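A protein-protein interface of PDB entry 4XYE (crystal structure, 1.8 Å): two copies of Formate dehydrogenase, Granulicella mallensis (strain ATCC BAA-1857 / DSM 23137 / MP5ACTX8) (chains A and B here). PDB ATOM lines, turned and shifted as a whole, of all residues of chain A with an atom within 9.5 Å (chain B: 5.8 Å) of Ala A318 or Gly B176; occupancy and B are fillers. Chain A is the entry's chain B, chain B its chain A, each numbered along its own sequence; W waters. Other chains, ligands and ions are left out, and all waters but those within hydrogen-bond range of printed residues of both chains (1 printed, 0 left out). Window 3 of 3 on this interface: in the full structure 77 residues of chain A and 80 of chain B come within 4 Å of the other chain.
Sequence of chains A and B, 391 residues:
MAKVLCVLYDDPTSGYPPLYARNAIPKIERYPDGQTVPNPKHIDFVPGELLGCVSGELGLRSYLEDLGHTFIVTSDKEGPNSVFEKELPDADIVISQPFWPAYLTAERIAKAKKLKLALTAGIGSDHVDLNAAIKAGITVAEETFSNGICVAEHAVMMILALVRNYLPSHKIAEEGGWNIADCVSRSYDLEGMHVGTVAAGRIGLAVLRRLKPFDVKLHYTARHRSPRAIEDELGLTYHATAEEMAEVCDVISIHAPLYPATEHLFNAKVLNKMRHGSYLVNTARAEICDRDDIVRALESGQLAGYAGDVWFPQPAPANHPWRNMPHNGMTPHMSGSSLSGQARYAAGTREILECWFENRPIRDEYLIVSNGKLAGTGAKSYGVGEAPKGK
Among the printed residues, merely in contact across the chains: Trp A311 with Ala B173, Trp A311 with Trp B178, Pro A315 with Trp B178, Ala A316 with Trp B178, Ala A318 with Gly B176, Arg A323 with Ile B172, Arg A323 with Gly B176, Pro A332 with Ile B172 and Pro A332 with Trp B178.
No position is printed for both chains.
Of the 12 pairs that touch across the chains among the printed residues, none has its exchanged pair printed and touching as well.
The side-chain amide oxygen (OD1) of Asn A324 sits close to the backbone carbonyl oxygen (O) of Glu B174, at 3.1 Å.
The backbone carbonyl oxygen (O) of Gly B177 sits at hydrogen-bond distance from the guanidinium group (NH1) of Arg A323.
The backbone carbonyl oxygen (O) of Ala B173 lies within hydrogen-bond range of the guanidinium group (NH1) of Arg A323.
Water W1 lies within hydrogen-bond range of the side-chain carboxylate of Glu B174 (2.9 Å) and the backbone carbonyl oxygen of Arg A323 (3.3 Å).
Hydrophobic or aromatic side chains of chain B within 4 Å of the printed part of chain A: Ile B172, Ala B173 and Trp B178.
Of the 13 printed residues of chain A, 7 touch a printed residue of chain B.
Printed residues of chain A that touch a printed residue of chain B: Trp A311, Pro A315, Ala A316, Ala A318, Arg A323, Asn A324 and Pro A332.
Hydrophobic or aromatic side chains of chain A that line the printed part of chain B: Trp A311, Pro A315, Ala A316, Ala A318 and Pro A332.
Among the printed residues, 12 pairs touch across the chains.
The backbone carbonyl oxygen (O) of Pro A317 lies within hydrogen-bond range of the guanidinium group (NE) of Arg A323, at 2.9 Å.
The backbone NH of Gly B177 sits at hydrogen-bond distance from the backbone carbonyl oxygen of Ile B172, 2.9 Å away.
NH2 of Arg A323 lies within hydrogen-bond range of O of Ala A316 (2.9 Å).
Printed residues of chain B within 4 Å of Trp A311: Ala B173 (3.98 Å) and Trp B178 (3.4 Å).
Of the printed residues of chain B, Pro A315 touches Trp B178 (3.6 Å).
Printed residues of chain B within 4 Å of Arg A323: Ile B172 (3.7 Å), Ala B173 (2.8 Å), Gly B176 (3.3 Å) and Gly B177 (2.8 Å).
Of the printed residues of chain B, Pro A332 touches Ile B172 and Trp B178.
Of the printed residues of chain A, Glu B174 touches Asn A324 (3.1 Å).
Gly B176 touches two residues of chain A.
The nearest printed residue of chain B that does not touch Ala A318 is Gly B177 (5.8 Å).
The nearest printed residue of chain A that does not touch Ile B172 is Trp A311 (7.1 Å).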
ATOM      1  N   TRP A 311     -29.264  10.803 -12.520  1.00  0.00           N
ATOM      2  CA  TRP A 311     -30.044   9.789 -13.225  1.00  0.00           C
ATOM      3  C   TRP A 311     -31.344   9.527 -12.470  1.00  0.00           C
ATOM      4  O   TRP A 311     -31.485   9.905 -11.309  1.00  0.00           O
ATOM      5  CB  TRP A 311     -29.277   8.460 -13.285  1.00  0.00           C
ATOM      6  CG  TRP A 311     -27.873   8.521 -13.815  1.00  0.00           C
ATOM      7  CD1 TRP A 311     -26.792   9.136 -13.231  1.00  0.00           C
ATOM      8  CD2 TRP A 311     -27.382   7.893 -15.000  1.00  0.00           C
ATOM      9  NE1 TRP A 311     -25.673   8.952 -14.002  1.00  0.00           N
ATOM     10  CE2 TRP A 311     -26.003   8.180 -15.083  1.00  0.00           C
ATOM     11  CE3 TRP A 311     -27.973   7.111 -16.002  1.00  0.00           C
ATOM     12  CZ2 TRP A 311     -25.213   7.722 -16.125  1.00  0.00           C
ATOM     13  CZ3 TRP A 311     -27.183   6.663 -17.039  1.00  0.00           C
ATOM     14  CH2 TRP A 311     -25.821   6.968 -17.098  1.00  0.00           C
ATOM     15  N   PRO A 313     -34.050   6.058 -11.888  1.00  0.00           N
ATOM     16  CA  PRO A 313     -33.763   6.217 -10.454  1.00  0.00           C
ATOM     17  C   PRO A 313     -32.261   6.108 -10.173  1.00  0.00           C
ATOM     18  O   PRO A 313     -31.483   5.879 -11.101  1.00  0.00           O
ATOM     19  CB  PRO A 313     -34.496   5.021  -9.826  1.00  0.00           C
ATOM     20  CG  PRO A 313     -34.426   3.956 -10.904  1.00  0.00           C
ATOM     21  CD  PRO A 313     -34.552   4.706 -12.215  1.00  0.00           C
ATOM     22  N   PRO A 315     -29.516   3.934  -7.742  1.00  0.00           N
ATOM     23  CA  PRO A 315     -28.629   3.839  -8.908  1.00  0.00           C
ATOM     24  C   PRO A 315     -29.367   3.545 -10.213  1.00  0.00           C
ATOM     25  O   PRO A 315     -30.430   2.910 -10.203  1.00  0.00           O
ATOM     26  CB  PRO A 315     -27.728   2.658  -8.554  1.00  0.00           C
ATOM     27  CG  PRO A 315     -28.608   1.789  -7.705  1.00  0.00           C
ATOM     28  CD  PRO A 315     -29.412   2.744  -6.875  1.00  0.00           C
ATOM     29  N   ALA A 316     -28.817   4.029 -11.322  1.00  0.00           N
ATOM     30  CA  ALA A 316     -29.401   3.752 -12.632  1.00  0.00           C
ATOM     31  C   ALA A 316     -29.245   2.270 -12.919  1.00  0.00           C
ATOM     32  O   ALA A 316     -28.157   1.719 -12.729  1.00  0.00           O
ATOM     33  CB  ALA A 316     -28.698   4.552 -13.691  1.00  0.00           C
ATOM     34  N   PRO A 317     -30.325   1.614 -13.378  1.00  0.00           N
ATOM     35  CA  PRO A 317     -30.216   0.215 -13.800  1.00  0.00           C
ATOM     36  C   PRO A 317     -29.170   0.053 -14.893  1.00  0.00           C
ATOM     37  O   PRO A 317     -28.886   1.011 -15.625  1.00  0.00           O
ATOM     38  CB  PRO A 317     -31.609  -0.093 -14.371  1.00  0.00           C
ATOM     39  CG  PRO A 317     -32.519   0.860 -13.676  1.00  0.00           C
ATOM     40  CD  PRO A 317     -31.709   2.113 -13.456  1.00  0.00           C
ATOM     41  N   ALA A 318     -28.618  -1.148 -15.022  1.00  0.00           N
ATOM     42  CA  ALA A 318     -27.580  -1.394 -16.023  1.00  0.00           C
ATOM     43  C   ALA A 318     -28.059  -1.141 -17.453  1.00  0.00           C
ATOM     44  O   ALA A 318     -27.242  -0.877 -18.335  1.00  0.00           O
ATOM     45  CB  ALA A 318     -27.009  -2.802 -15.889  1.00  0.00           C
ATOM     46  N   ASN A 319     -29.372  -1.200 -17.672  1.00  0.00           N
ATOM     47  CA  ASN A 319     -29.940  -1.017 -19.009  1.00  0.00           C
ATOM     48  C   ASN A 319     -30.558   0.373 -19.225  1.00  0.00           C
ATOM     49  O   ASN A 319     -31.303   0.597 -20.193  1.00  0.00           O
ATOM     50  CB  ASN A 319     -30.980  -2.103 -19.301  1.00  0.00           C
ATOM     51  CG  ASN A 319     -32.297  -1.867 -18.580  1.00  0.00           C
ATOM     52  OD1 ASN A 319     -32.366  -1.136 -17.588  1.00  0.00           O
ATOM     53  ND2 ASN A 319     -33.354  -2.492 -19.077  1.00  0.00           N
ATOM     54  N   HIS A 320     -30.256   1.297 -18.318  1.00  0.00           N
ATOM     55  CA  HIS A 320     -30.801   2.644 -18.388  1.00  0.00           C
ATOM     56  C   HIS A 320     -30.379   3.256 -19.724  1.00  0.00           C
ATOM     57  O   HIS A 320     -29.201   3.192 -20.087  1.00  0.00           O
ATOM     58  CB  HIS A 320     -30.274   3.473 -17.209  1.00  0.00           C
ATOM     59  CG  HIS A 320     -30.928   4.811 -17.084  1.00  0.00           C
ATOM     60  ND1 HIS A 320     -30.774   5.798 -18.030  1.00  0.00           N
ATOM     61  CD2 HIS A 320     -31.742   5.319 -16.127  1.00  0.00           C
ATOM     62  CE1 HIS A 320     -31.456   6.871 -17.654  1.00  0.00           C
ATOM     63  NE2 HIS A 320     -32.062   6.599 -16.515  1.00  0.00           N
ATOM     64  N   PRO A 321     -31.342   3.825 -20.477  1.00  0.00           N
ATOM     65  CA  PRO A 321     -31.046   4.321 -21.834  1.00  0.00           C
ATOM     66  C   PRO A 321     -30.031   5.481 -21.924  1.00  0.00           C
ATOM     67  O   PRO A 321     -29.481   5.702 -22.995  1.00  0.00           O
ATOM     68  CB  PRO A 321     -32.421   4.774 -22.353  1.00  0.00           C
ATOM     69  CG  PRO A 321     -33.227   5.047 -21.115  1.00  0.00           C
ATOM     70  CD  PRO A 321     -32.765   3.994 -20.133  1.00  0.00           C
ATOM     71  N   TRP A 322     -29.780   6.207 -20.841  1.00  0.00           N
ATOM     72  CA  TRP A 322     -28.806   7.306 -20.903  1.00  0.00           C
ATOM     73  C   TRP A 322     -27.356   6.814 -20.978  1.00  0.00           C
ATOM     74  O   TRP A 322     -26.449   7.570 -21.316  1.00  0.00           O
ATOM     75  CB  TRP A 322     -28.999   8.277 -19.723  1.00  0.00           C
ATOM     76  CG  TRP A 322     -30.173   9.202 -19.888  1.00  0.00           C
ATOM     77  CD1 TRP A 322     -31.082   9.206 -20.909  1.00  0.00           C
ATOM     78  CD2 TRP A 322     -30.559  10.263 -19.005  1.00  0.00           C
ATOM     79  NE1 TRP A 322     -32.011  10.206 -20.715  1.00  0.00           N
ATOM     80  CE2 TRP A 322     -31.708  10.871 -19.558  1.00  0.00           C
ATOM     81  CE3 TRP A 322     -30.047  10.752 -17.797  1.00  0.00           C
ATOM     82  CZ2 TRP A 322     -32.350  11.947 -18.945  1.00  0.00           C
ATOM     83  CZ3 TRP A 322     -30.689  11.818 -17.182  1.00  0.00           C
ATOM     84  CH2 TRP A 322     -31.827  12.411 -17.762  1.00  0.00           C
ATOM     85  N   ARG A 323     -27.135   5.541 -20.671  1.00  0.00           N
ATOM     86  CA  ARG A 323     -25.777   5.005 -20.662  1.00  0.00           C
ATOM     87  C   ARG A 323     -25.157   4.938 -22.048  1.00  0.00           C
ATOM     88  O   ARG A 323     -23.993   5.279 -22.228  1.00  0.00           O
ATOM     89  CB  ARG A 323     -25.747   3.616 -20.022  1.00  0.00           C
ATOM     90  CG  ARG A 323     -26.113   3.608 -18.555  1.00  0.00           C
ATOM     91  CD  ARG A 323     -26.062   2.179 -18.030  1.00  0.00           C
ATOM     92  NE  ARG A 323     -26.361   2.098 -16.603  1.00  0.00           N
ATOM     93  CZ  ARG A 323     -25.475   2.307 -15.636  1.00  0.00           C
ATOM     94  NH1 ARG A 323     -24.219   2.630 -15.930  1.00  0.00           N
ATOM     95  NH2 ARG A 323     -25.848   2.196 -14.369  1.00  0.00           N
ATOM     96  N   ASN A 324     -25.936   4.511 -23.034  1.00  0.00           N
ATOM     97  CA  ASN A 324     -25.362   4.251 -24.347  1.00  0.00           C
ATOM     98  C   ASN A 324     -26.036   5.009 -25.486  1.00  0.00           C
ATOM     99  O   ASN A 324     -25.781   4.732 -26.655  1.00  0.00           O
ATOM    100  CB  ASN A 324     -25.339   2.746 -24.628  1.00  0.00           C
ATOM    101  CG  ASN A 324     -24.600   1.969 -23.544  1.00  0.00           C
ATOM    102  OD1 ASN A 324     -23.402   2.171 -23.328  1.00  0.00           O
ATOM    103  ND2 ASN A 324     -25.316   1.082 -22.851  1.00  0.00           N
ATOM    104  N   PRO A 332     -21.617   8.262 -13.430  1.00  0.00           N
ATOM    105  CA  PRO A 332     -22.534   8.002 -12.312  1.00  0.00           C
ATOM    106  C   PRO A 332     -22.630   9.262 -11.436  1.00  0.00           C
ATOM    107  O   PRO A 332     -21.856  10.193 -11.649  1.00  0.00           O
ATOM    108  CB  PRO A 332     -21.841   6.862 -11.549  1.00  0.00           C
ATOM    109  CG  PRO A 332     -20.967   6.188 -12.584  1.00  0.00           C
ATOM    110  CD  PRO A 332     -20.476   7.331 -13.443  1.00  0.00           C
ATOM    111  N   LYS B 171     -16.454   5.703 -18.340  1.00  0.00           N
ATOM    112  CA  LYS B 171     -16.369   4.309 -18.785  1.00  0.00           C
ATOM    113  C   LYS B 171     -17.295   3.421 -17.945  1.00  0.00           C
ATOM    114  O   LYS B 171     -17.980   2.546 -18.473  1.00  0.00           O
ATOM    115  CB  LYS B 171     -14.922   3.832 -18.700  1.00  0.00           C
ATOM    116  CG  LYS B 171     -14.648   2.421 -19.203  1.00  0.00           C
ATOM    117  CD  LYS B 171     -13.141   2.207 -19.371  1.00  0.00           C
ATOM    118  CE  LYS B 171     -12.765   0.727 -19.398  1.00  0.00           C
ATOM    119  NZ  LYS B 171     -12.904   0.093 -18.053  1.00  0.00           N
ATOM    120  N   ILE B 172     -17.318   3.671 -16.639  1.00  0.00           N
ATOM    121  CA  ILE B 172     -18.232   2.973 -15.741  1.00  0.00           C
ATOM    122  C   ILE B 172     -19.701   3.210 -16.111  1.00  0.00           C
ATOM    123  O   ILE B 172     -20.500   2.271 -16.125  1.00  0.00           O
ATOM    124  CB  ILE B 172     -17.968   3.333 -14.263  1.00  0.00           C
ATOM    125  CG1 ILE B 172     -16.650   2.694 -13.808  1.00  0.00           C
ATOM    126  CG2 ILE B 172     -19.125   2.855 -13.376  1.00  0.00           C
ATOM    127  CD1 ILE B 172     -16.147   3.197 -12.466  1.00  0.00           C
ATOM    128  N   ALA B 173     -20.057   4.450 -16.445  1.00  0.00           N
ATOM    129  CA  ALA B 173     -21.425   4.717 -16.887  1.00  0.00           C
ATOM    130  C   ALA B 173     -21.734   3.914 -18.155  1.00  0.00           C
ATOM    131  O   ALA B 173     -22.765   3.228 -18.232  1.00  0.00           O
ATOM    132  CB  ALA B 173     -21.662   6.213 -17.119  1.00  0.00           C
ATOM    133  N   GLU B 174     -20.833   3.980 -19.130  1.00  0.00           N
ATOM    134  CA  GLU B 174     -21.008   3.246 -20.384  1.00  0.00           C
ATOM    135  C   GLU B 174     -21.130   1.732 -20.174  1.00  0.00           C
ATOM    136  O   GLU B 174     -21.871   1.059 -20.896  1.00  0.00           O
ATOM    137  CB  GLU B 174     -19.837   3.499 -21.331  1.00  0.00           C
ATOM    138  CG  GLU B 174     -19.701   4.903 -21.844  1.00  0.00           C
ATOM    139  CD  GLU B 174     -18.532   5.031 -22.823  1.00  0.00           C
ATOM    140  OE1 GLU B 174     -17.356   4.963 -22.381  1.00  0.00           O
ATOM    141  OE2 GLU B 174     -18.788   5.176 -24.040  1.00  0.00           O
ATOM    142  N   GLU B 175     -20.388   1.202 -19.203  1.00  0.00           N
ATOM    143  CA  GLU B 175     -20.296  -0.242 -18.997  1.00  0.00           C
ATOM    144  C   GLU B 175     -21.414  -0.813 -18.137  1.00  0.00           C
ATOM    145  O   GLU B 175     -21.494  -2.029 -17.948  1.00  0.00           O
ATOM    146  CB  GLU B 175     -18.959  -0.619 -18.358  1.00  0.00           C
ATOM    147  CG  GLU B 175     -17.776  -0.579 -19.281  1.00  0.00           C
ATOM    148  CD  GLU B 175     -16.474  -0.728 -18.509  1.00  0.00           C
ATOM    149  OE1 GLU B 175     -16.501  -0.579 -17.260  1.00  0.00           O
ATOM    150  OE2 GLU B 175     -15.432  -0.993 -19.140  1.00  0.00           O
ATOM    151  N   GLY B 176     -22.264   0.046 -17.593  1.00  0.00           N
ATOM    152  CA  GLY B 176     -23.392  -0.452 -16.825  1.00  0.00           C
ATOM    153  C   GLY B 176     -23.191  -0.424 -15.319  1.00  0.00           C
ATOM    154  O   GLY B 176     -24.020  -0.936 -14.577  1.00  0.00           O
ATOM    155  N   GLY B 177     -22.094   0.174 -14.869  1.00  0.00           N
ATOM    156  CA  GLY B 177     -21.802   0.257 -13.447  1.00  0.00           C
ATOM    157  C   GLY B 177     -22.406   1.482 -12.779  1.00  0.00           C
ATOM    158  O   GLY B 177     -23.137   2.257 -13.401  1.00  0.00           O
ATOM    159  N   TRP B 178     -22.103   1.633 -11.497  1.00  0.00           N
ATOM    160  CA  TRP B 178     -22.470   2.806 -10.722  1.00  0.00           C
ATOM    161  C   TRP B 178     -21.245   3.110  -9.869  1.00  0.00           C
ATOM    162  O   TRP B 178     -20.504   4.051 -10.150  1.00  0.00           O
ATOM    163  CB  TRP B 178     -23.721   2.537  -9.880  1.00  0.00           C
ATOM    164  CG  TRP B 178     -24.334   3.767  -9.220  1.00  0.00           C
ATOM    165  CD1 TRP B 178     -24.346   4.062  -7.882  1.00  0.00           C
ATOM    166  CD2 TRP B 178     -25.031   4.841  -9.869  1.00  0.00           C
ATOM    167  NE1 TRP B 178     -25.016   5.246  -7.657  1.00  0.00           N
ATOM    168  CE2 TRP B 178     -25.438   5.748  -8.862  1.00  0.00           C
ATOM    169  CE3 TRP B 178     -25.362   5.120 -11.204  1.00  0.00           C
ATOM    170  CZ2 TRP B 178     -26.138   6.921  -9.150  1.00  0.00           C
ATOM    171  CZ3 TRP B 178     -26.060   6.285 -11.489  1.00  0.00           C
ATOM    172  CH2 TRP B 178     -26.441   7.171 -10.467  1.00  0.00           C
HETATM  173  O   HOH W   1     -21.367   6.462 -23.773  1.00  0.00           O
